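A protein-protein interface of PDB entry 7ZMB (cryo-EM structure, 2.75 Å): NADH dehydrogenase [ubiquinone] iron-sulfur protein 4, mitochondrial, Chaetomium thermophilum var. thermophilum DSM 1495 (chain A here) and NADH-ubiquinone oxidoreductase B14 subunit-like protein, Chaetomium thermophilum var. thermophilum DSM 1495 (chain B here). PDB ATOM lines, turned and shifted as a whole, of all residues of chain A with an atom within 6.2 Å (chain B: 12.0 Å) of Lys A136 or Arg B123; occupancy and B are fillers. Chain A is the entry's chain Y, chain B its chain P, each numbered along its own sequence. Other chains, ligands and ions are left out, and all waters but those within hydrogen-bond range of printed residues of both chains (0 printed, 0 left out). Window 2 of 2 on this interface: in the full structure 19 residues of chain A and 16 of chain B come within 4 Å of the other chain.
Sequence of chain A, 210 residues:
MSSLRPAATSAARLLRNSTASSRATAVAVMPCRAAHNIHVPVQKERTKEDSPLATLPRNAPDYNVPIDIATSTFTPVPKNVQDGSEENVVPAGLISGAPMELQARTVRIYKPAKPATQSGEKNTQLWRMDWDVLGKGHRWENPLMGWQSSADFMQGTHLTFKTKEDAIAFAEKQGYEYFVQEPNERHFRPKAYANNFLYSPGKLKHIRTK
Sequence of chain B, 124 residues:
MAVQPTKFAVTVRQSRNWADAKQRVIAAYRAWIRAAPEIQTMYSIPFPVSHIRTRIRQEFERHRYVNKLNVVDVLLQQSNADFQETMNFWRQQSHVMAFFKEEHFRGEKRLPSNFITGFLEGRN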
ATOM      1  N   THR A  73      17.394  14.200  24.001  1.00  0.00           N
ATOM      2  CA  THR A  73      16.473  13.165  23.574  1.00  0.00           C
ATOM      3  C   THR A  73      16.337  13.088  22.062  1.00  0.00           C
ATOM      4  O   THR A  73      15.580  12.253  21.568  1.00  0.00           O
ATOM      5  CB  THR A  73      15.099  13.381  24.214  1.00  0.00           C
ATOM      6  OG1 THR A  73      14.244  12.276  23.898  1.00  0.00           O
ATOM      7  CG2 THR A  73      14.476  14.680  23.735  1.00  0.00           C
ATOM      8  N   PHE A  74      17.042  13.938  21.318  1.00  0.00           N
ATOM      9  CA  PHE A  74      17.019  13.910  19.863  1.00  0.00           C
ATOM     10  C   PHE A  74      18.365  13.500  19.277  1.00  0.00           C
ATOM     11  O   PHE A  74      18.576  13.638  18.070  1.00  0.00           O
ATOM     12  CB  PHE A  74      16.603  15.267  19.295  1.00  0.00           C
ATOM     13  CG  PHE A  74      15.390  15.853  19.936  1.00  0.00           C
ATOM     14  CD1 PHE A  74      14.123  15.490  19.518  1.00  0.00           C
ATOM     15  CD2 PHE A  74      15.513  16.790  20.941  1.00  0.00           C
ATOM     16  CE1 PHE A  74      13.009  16.032  20.099  1.00  0.00           C
ATOM     17  CE2 PHE A  74      14.402  17.340  21.521  1.00  0.00           C
ATOM     18  CZ  PHE A  74      13.148  16.959  21.100  1.00  0.00           C
ATOM     19  N   THR A  75      19.277  13.015  20.099  1.00  0.00           N
ATOM     20  CA  THR A  75      20.579  12.594  19.600  1.00  0.00           C
ATOM     21  C   THR A  75      20.471  11.192  19.008  1.00  0.00           C
ATOM     22  O   THR A  75      19.906  10.303  19.644  1.00  0.00           O
ATOM     23  CB  THR A  75      21.617  12.622  20.721  1.00  0.00           C
ATOM     24  OG1 THR A  75      21.724  13.952  21.241  1.00  0.00           O
ATOM     25  CG2 THR A  75      22.973  12.212  20.200  1.00  0.00           C
ATOM     26  N   PRO A  76      20.961  10.966  17.795  1.00  0.00           N
ATOM     27  CA  PRO A  76      20.882   9.627  17.209  1.00  0.00           C
ATOM     28  C   PRO A  76      21.842   8.654  17.871  1.00  0.00           C
ATOM     29  O   PRO A  76      22.842   9.043  18.480  1.00  0.00           O
ATOM     30  CB  PRO A  76      21.266   9.856  15.742  1.00  0.00           C
ATOM     31  CG  PRO A  76      21.221  11.322  15.538  1.00  0.00           C
ATOM     32  CD  PRO A  76      21.527  11.938  16.853  1.00  0.00           C
ATOM     33  N   VAL A  77      21.522   7.372  17.752  1.00  0.00           N
ATOM     34  CA  VAL A  77      22.476   6.334  18.155  1.00  0.00           C
ATOM     35  C   VAL A  77      23.605   6.270  17.132  1.00  0.00           C
ATOM     36  O   VAL A  77      23.342   6.260  15.918  1.00  0.00           O
ATOM     37  CB  VAL A  77      21.771   4.982  18.302  1.00  0.00           C
ATOM     38  CG1 VAL A  77      20.721   5.058  19.392  1.00  0.00           C
ATOM     39  CG2 VAL A  77      21.100   4.573  16.991  1.00  0.00           C
ATOM     40  N   GLU A 101      27.132  13.474  18.682  1.00  0.00           N
ATOM     41  CA  GLU A 101      26.041  13.534  17.723  1.00  0.00           C
ATOM     42  C   GLU A 101      26.536  13.872  16.324  1.00  0.00           C
ATOM     43  O   GLU A 101      25.864  13.549  15.344  1.00  0.00           O
ATOM     44  CB  GLU A 101      25.004  14.558  18.201  1.00  0.00           C
ATOM     45  CG  GLU A 101      23.789  14.701  17.306  1.00  0.00           C
ATOM     46  CD  GLU A 101      22.630  15.400  17.984  1.00  0.00           C
ATOM     47  OE1 GLU A 101      22.717  15.655  19.204  1.00  0.00           O
ATOM     48  OE2 GLU A 101      21.631  15.698  17.295  1.00  0.00           O
ATOM     49  N   LEU A 134      16.426  15.219  10.864  1.00  0.00           N
ATOM     50  CA  LEU A 134      16.060  14.047  11.641  1.00  0.00           C
ATOM     51  C   LEU A 134      14.555  14.032  11.862  1.00  0.00           C
ATOM     52  O   LEU A 134      13.880  15.051  11.712  1.00  0.00           O
ATOM     53  CB  LEU A 134      16.791  14.027  12.979  1.00  0.00           C
ATOM     54  CG  LEU A 134      18.306  14.196  12.897  1.00  0.00           C
ATOM     55  CD1 LEU A 134      18.942  14.036  14.253  1.00  0.00           C
ATOM     56  CD2 LEU A 134      18.908  13.220  11.905  1.00  0.00           C
ATOM     57  N   GLY A 135      14.036  12.860  12.222  1.00  0.00           N
ATOM     58  CA  GLY A 135      12.595  12.682  12.271  1.00  0.00           C
ATOM     59  C   GLY A 135      11.925  13.508  13.350  1.00  0.00           C
ATOM     60  O   GLY A 135      10.833  14.040  13.151  1.00  0.00           O
ATOM     61  N   LYS A 136      12.560  13.615  14.509  1.00  0.00           N
ATOM     62  CA  LYS A 136      12.057  14.436  15.599  1.00  0.00           C
ATOM     63  C   LYS A 136      13.031  15.551  15.945  1.00  0.00           C
ATOM     64  O   LYS A 136      14.249  15.399  15.812  1.00  0.00           O
ATOM     65  CB  LYS A 136      11.769  13.595  16.844  1.00  0.00           C
ATOM     66  CG  LYS A 136      10.729  12.520  16.645  1.00  0.00           C
ATOM     67  CD  LYS A 136       9.372  13.164  16.364  1.00  0.00           C
ATOM     68  CE  LYS A 136       8.242  12.154  16.320  1.00  0.00           C
ATOM     69  NZ  LYS A 136       8.327  11.261  15.147  1.00  0.00           N
ATOM     70  N   GLY A 137      12.480  16.679  16.381  1.00  0.00           N
ATOM     71  CA  GLY A 137      13.260  17.770  16.906  1.00  0.00           C
ATOM     72  C   GLY A 137      13.699  18.819  15.910  1.00  0.00           C
ATOM     73  O   GLY A 137      14.302  19.814  16.325  1.00  0.00           O
ATOM     74  N   HIS A 138      13.437  18.635  14.613  1.00  0.00           N
ATOM     75  CA  HIS A 138      13.864  19.637  13.642  1.00  0.00           C
ATOM     76  C   HIS A 138      13.030  20.903  13.755  1.00  0.00           C
ATOM     77  O   HIS A 138      13.578  22.008  13.737  1.00  0.00           O
ATOM     78  CB  HIS A 138      13.805  19.074  12.225  1.00  0.00           C
ATOM     79  CG  HIS A 138      14.247  20.044  11.172  1.00  0.00           C
ATOM     80  ND1 HIS A 138      13.409  20.496  10.178  1.00  0.00           N
ATOM     81  CD2 HIS A 138      15.440  20.646  10.960  1.00  0.00           C
ATOM     82  CE1 HIS A 138      14.066  21.336   9.401  1.00  0.00           C
ATOM     83  NE2 HIS A 138      15.300  21.446   9.855  1.00  0.00           N
ATOM     84  N   ARG A 139      11.712  20.763  13.877  1.00  0.00           N
ATOM     85  CA  ARG A 139      10.815  21.889  14.097  1.00  0.00           C
ATOM     86  C   ARG A 139       9.608  21.409  14.883  1.00  0.00           C
ATOM     87  O   ARG A 139       9.129  20.292  14.691  1.00  0.00           O
ATOM     88  CB  ARG A 139      10.334  22.533  12.786  1.00  0.00           C
ATOM     89  CG  ARG A 139      11.365  23.292  11.983  1.00  0.00           C
ATOM     90  CD  ARG A 139      11.856  24.533  12.697  1.00  0.00           C
ATOM     91  NE  ARG A 139      12.662  25.371  11.820  1.00  0.00           N
ATOM     92  CZ  ARG A 139      13.936  25.147  11.528  1.00  0.00           C
ATOM     93  NH1 ARG A 139      14.580  25.961  10.713  1.00  0.00           N
ATOM     94  NH2 ARG A 139      14.566  24.113  12.044  1.00  0.00           N
ATOM     95  N   LEU B 111      21.024   7.722  25.795  1.00  0.00           N
ATOM     96  CA  LEU B 111      20.659   7.015  24.574  1.00  0.00           C
ATOM     97  C   LEU B 111      19.981   5.689  24.899  1.00  0.00           C
ATOM     98  O   LEU B 111      20.375   5.007  25.844  1.00  0.00           O
ATOM     99  CB  LEU B 111      21.893   6.782  23.701  1.00  0.00           C
ATOM    100  CG  LEU B 111      22.536   8.040  23.119  1.00  0.00           C
ATOM    101  CD1 LEU B 111      23.844   7.704  22.427  1.00  0.00           C
ATOM    102  CD2 LEU B 111      21.582   8.738  22.157  1.00  0.00           C
ATOM    103  N   PRO B 112      18.957   5.331  24.124  1.00  0.00           N
ATOM    104  CA  PRO B 112      18.237   4.081  24.387  1.00  0.00           C
ATOM    105  C   PRO B 112      19.156   2.876  24.265  1.00  0.00           C
ATOM    106  O   PRO B 112      20.045   2.834  23.413  1.00  0.00           O
ATOM    107  CB  PRO B 112      17.139   4.066  23.314  1.00  0.00           C
ATOM    108  CG  PRO B 112      17.609   5.006  22.258  1.00  0.00           C
ATOM    109  CD  PRO B 112      18.412   6.055  22.963  1.00  0.00           C
ATOM    110  N   SER B 113      18.934   1.891  25.134  1.00  0.00           N
ATOM    111  CA  SER B 113      19.784   0.708  25.179  1.00  0.00           C
ATOM    112  C   SER B 113      19.422  -0.324  24.121  1.00  0.00           C
ATOM    113  O   SER B 113      20.186  -1.273  23.922  1.00  0.00           O
ATOM    114  CB  SER B 113      19.716   0.069  26.568  1.00  0.00           C
ATOM    115  OG  SER B 113      20.727  -0.910  26.730  1.00  0.00           O
ATOM    116  N   ASN B 114      18.291  -0.159  23.443  1.00  0.00           N
ATOM    117  CA  ASN B 114      17.840  -1.081  22.414  1.00  0.00           C
ATOM    118  C   ASN B 114      17.110  -0.295  21.339  1.00  0.00           C
ATOM    119  O   ASN B 114      16.695   0.845  21.553  1.00  0.00           O
ATOM    120  CB  ASN B 114      16.919  -2.161  22.983  1.00  0.00           C
ATOM    121  CG  ASN B 114      17.669  -3.201  23.779  1.00  0.00           C
ATOM    122  OD1 ASN B 114      17.553  -3.268  25.004  1.00  0.00           O
ATOM    123  ND2 ASN B 114      18.441  -4.030  23.088  1.00  0.00           N
ATOM    124  N   PHE B 115      16.966  -0.913  20.167  1.00  0.00           N
ATOM    125  CA  PHE B 115      16.162  -0.302  19.117  1.00  0.00           C
ATOM    126  C   PHE B 115      14.717  -0.162  19.562  1.00  0.00           C
ATOM    127  O   PHE B 115      14.089   0.880  19.353  1.00  0.00           O
ATOM    128  CB  PHE B 115      16.243  -1.123  17.826  1.00  0.00           C
ATOM    129  CG  PHE B 115      15.225  -0.720  16.797  1.00  0.00           C
ATOM    130  CD1 PHE B 115      13.934  -1.228  16.833  1.00  0.00           C
ATOM    131  CD2 PHE B 115      15.551   0.185  15.803  1.00  0.00           C
ATOM    132  CE1 PHE B 115      12.995  -0.830  15.913  1.00  0.00           C
ATOM    133  CE2 PHE B 115      14.605   0.573  14.871  1.00  0.00           C
ATOM    134  CZ  PHE B 115      13.331   0.065  14.931  1.00  0.00           C
ATOM    135  N   ILE B 116      14.166  -1.212  20.168  1.00  0.00           N
ATOM    136  CA  ILE B 116      12.747  -1.221  20.490  1.00  0.00           C
ATOM    137  C   ILE B 116      12.445  -0.211  21.586  1.00  0.00           C
ATOM    138  O   ILE B 116      11.399   0.445  21.569  1.00  0.00           O
ATOM    139  CB  ILE B 116      12.292  -2.648  20.857  1.00  0.00           C
ATOM    140  CG1 ILE B 116      10.826  -2.673  21.299  1.00  0.00           C
ATOM    141  CG2 ILE B 116      13.179  -3.240  21.922  1.00  0.00           C
ATOM    142  CD1 ILE B 116       9.853  -2.282  20.223  1.00  0.00           C
ATOM    143  N   THR B 117      13.354  -0.062  22.552  1.00  0.00           N
ATOM    144  CA  THR B 117      13.191   0.977  23.564  1.00  0.00           C
ATOM    145  C   THR B 117      13.234   2.359  22.932  1.00  0.00           C
ATOM    146  O   THR B 117      12.419   3.228  23.253  1.00  0.00           O
ATOM    147  CB  THR B 117      14.265   0.850  24.639  1.00  0.00           C
ATOM    148  OG1 THR B 117      14.164  -0.430  25.270  1.00  0.00           O
ATOM    149  CG2 THR B 117      14.098   1.925  25.686  1.00  0.00           C
ATOM    150  N   GLY B 118      14.180   2.573  22.021  1.00  0.00           N
ATOM    151  CA  GLY B 118      14.239   3.841  21.315  1.00  0.00           C
ATOM    152  C   GLY B 118      13.013   4.096  20.464  1.00  0.00           C
ATOM    153  O   GLY B 118      12.525   5.220  20.390  1.00  0.00           O
ATOM    154  N   PHE B 119      12.500   3.056  19.809  1.00  0.00           N
ATOM    155  CA  PHE B 119      11.355   3.246  18.924  1.00  0.00           C
ATOM    156  C   PHE B 119      10.124   3.682  19.697  1.00  0.00           C
ATOM    157  O   PHE B 119       9.379   4.555  19.247  1.00  0.00           O
ATOM    158  CB  PHE B 119      11.059   1.961  18.152  1.00  0.00           C
ATOM    159  CG  PHE B 119       9.806   2.028  17.330  1.00  0.00           C
ATOM    160  CD1 PHE B 119       9.831   2.537  16.044  1.00  0.00           C
ATOM    161  CD2 PHE B 119       8.600   1.583  17.840  1.00  0.00           C
ATOM    162  CE1 PHE B 119       8.678   2.595  15.289  1.00  0.00           C
ATOM    163  CE2 PHE B 119       7.449   1.652  17.088  1.00  0.00           C
ATOM    164  CZ  PHE B 119       7.489   2.151  15.811  1.00  0.00           C
ATOM    165  N   LEU B 120       9.892   3.079  20.860  1.00  0.00           N
ATOM    166  CA  LEU B 120       8.617   3.240  21.543  1.00  0.00           C
ATOM    167  C   LEU B 120       8.490   4.597  22.216  1.00  0.00           C
ATOM    168  O   LEU B 120       7.373   5.075  22.430  1.00  0.00           O
ATOM    169  CB  LEU B 120       8.436   2.119  22.560  1.00  0.00           C
ATOM    170  CG  LEU B 120       8.071   0.756  21.982  1.00  0.00           C
ATOM    171  CD1 LEU B 120       7.796  -0.228  23.095  1.00  0.00           C
ATOM    172  CD2 LEU B 120       6.876   0.856  21.047  1.00  0.00           C
ATOM    173  N   GLU B 121       9.604   5.230  22.557  1.00  0.00           N
ATOM    174  CA  GLU B 121       9.581   6.513  23.238  1.00  0.00           C
ATOM    175  C   GLU B 121       9.707   7.702  22.295  1.00  0.00           C
ATOM    176  O   GLU B 121       9.842   8.832  22.767  1.00  0.00           O
ATOM    177  CB  GLU B 121      10.705   6.568  24.276  1.00  0.00           C
ATOM    178  CG  GLU B 121      10.535   5.614  25.438  1.00  0.00           C
ATOM    179  CD  GLU B 121      11.676   5.688  26.436  1.00  0.00           C
ATOM    180  OE1 GLU B 121      12.666   6.395  26.159  1.00  0.00           O
ATOM    181  OE2 GLU B 121      11.579   5.042  27.501  1.00  0.00           O
ATOM    182  N   GLY B 122       9.654   7.485  20.989  1.00  0.00           N
ATOM    183  CA  GLY B 122      10.261   8.407  20.055  1.00  0.00           C
ATOM    184  C   GLY B 122      11.768   8.239  20.070  1.00  0.00           C
ATOM    185  O   GLY B 122      12.342   7.679  20.997  1.00  0.00           O
ATOM    186  N   ARG B 123      12.422   8.721  19.013  1.00  0.00           N
ATOM    187  CA  ARG B 123      13.849   8.450  18.858  1.00  0.00           C
ATOM    188  C   ARG B 123      14.587   8.849  20.122  1.00  0.00           C
ATOM    189  O   ARG B 123      14.692  10.034  20.439  1.00  0.00           O
ATOM    190  CB  ARG B 123      14.419   9.203  17.659  1.00  0.00           C
ATOM    191  CG  ARG B 123      15.829   8.788  17.323  1.00  0.00           C
ATOM    192  CD  ARG B 123      16.356   9.505  16.111  1.00  0.00           C
ATOM    193  NE  ARG B 123      16.723  10.889  16.396  1.00  0.00           N
ATOM    194  CZ  ARG B 123      15.995  11.944  16.054  1.00  0.00           C
ATOM    195  NH1 ARG B 123      14.844  11.791  15.418  1.00  0.00           N
ATOM    196  NH2 ARG B 123      16.421  13.156  16.359  1.00  0.00           N
ATOM    197  N   ASN B 124      15.094   7.851  20.837  1.00  0.00           N
ATOM    198  CA  ASN B 124      15.418   7.993  22.256  1.00  0.00           C
ATOM    199  C   ASN B 124      14.169   8.395  23.030  1.00  0.00           C
ATOM    200  O   ASN B 124      13.674   9.516  22.924  1.00  0.00           O
ATOM    201  CB  ASN B 124      16.534   9.013  22.491  1.00  0.00           C
ATOM    202  CG  ASN B 124      16.854   9.189  23.947  1.00  0.00           C
ATOM    203  OD1 ASN B 124      16.474   8.373  24.782  1.00  0.00           O
ATOM    204  ND2 ASN B 124      17.568  10.251  24.264  1.00  0.00           N
ATOM    205  OXT ASN B 124      13.618   7.595  23.784  1.00  0.00           O
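Of chain B, only Arg B123 (2.6 Å) and Asn B124 (3.0 Å) come within 4 Å of Thr A73.
Thr A75 touches one residue of chain B.
Of chain B, only Leu B111 comes within 4 Å of Pro A76.
Gly A137 touches none of the printed residues of chain B.
Printed residues of chain A within 4 Å of Asn B124: Thr A73 (3.0 Å).
Printed residues of chain A within 4 Å of Leu B111: Thr A75 (3.4 Å) and Pro A76 (3.9 Å).
Gly B118 touches none of the printed residues of chain A.
Val A77 touches none of the printed residues of chain B.
The nearest residue of chain B that does not touch Lys A136 is Gly B122 (5.4 Å).
The nearest residue of chain A that does not touch Arg B123 is Pro A76 (4.4 Å).
The nearest printed residue of chain A that does not touch Asn B124 is Thr A75 (4.6 Å).
Hydrophobic or aromatic side chains of chain A within 4 Å of the printed part of chain B: Phe A74 and Leu A134.
Hydrophobic or aromatic side chains of chain B within 4 Å of the printed part of chain A: Leu B111.
Among the printed residues, 8 pairs touch across the chains.
Among the printed residues, no Asp or Glu carboxylate lies within 4 Å of a Lys or Arg side-chain nitrogen of the other chain.
Among the printed residues, merely in contact across the chains: Leu A134 with Arg B123 (3.4 Å), Thr A75 with Leu B111 (3.4 Å) and Pro A76 with Leu B111 (3.9 Å).
The side-chain hydroxyl (OG1) of Thr A73 sits at hydrogen-bond distance from the chain-end carboxylate (O) of Asn B124 (3.0 Å).
N of Gly A135 sits close to NH1 of Arg B123 (3.5 Å).
The guanidinium group of Arg B123 lies within hydrogen-bond range of the backbone carbonyl oxygen of Lys A136 (3.2 Å).
The backbone carbonyl oxygen of Arg B123 lies close to the backbone carbonyl oxygen of Thr A73 (2.6 Å).
O of Phe A74 lies within hydrogen-bond range of NH2 of Arg B123, 2.8 Å away.
OG1 of Thr A75 lies within hydrogen-bond range of OE1 of Glu A101, 2.8 Å away.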
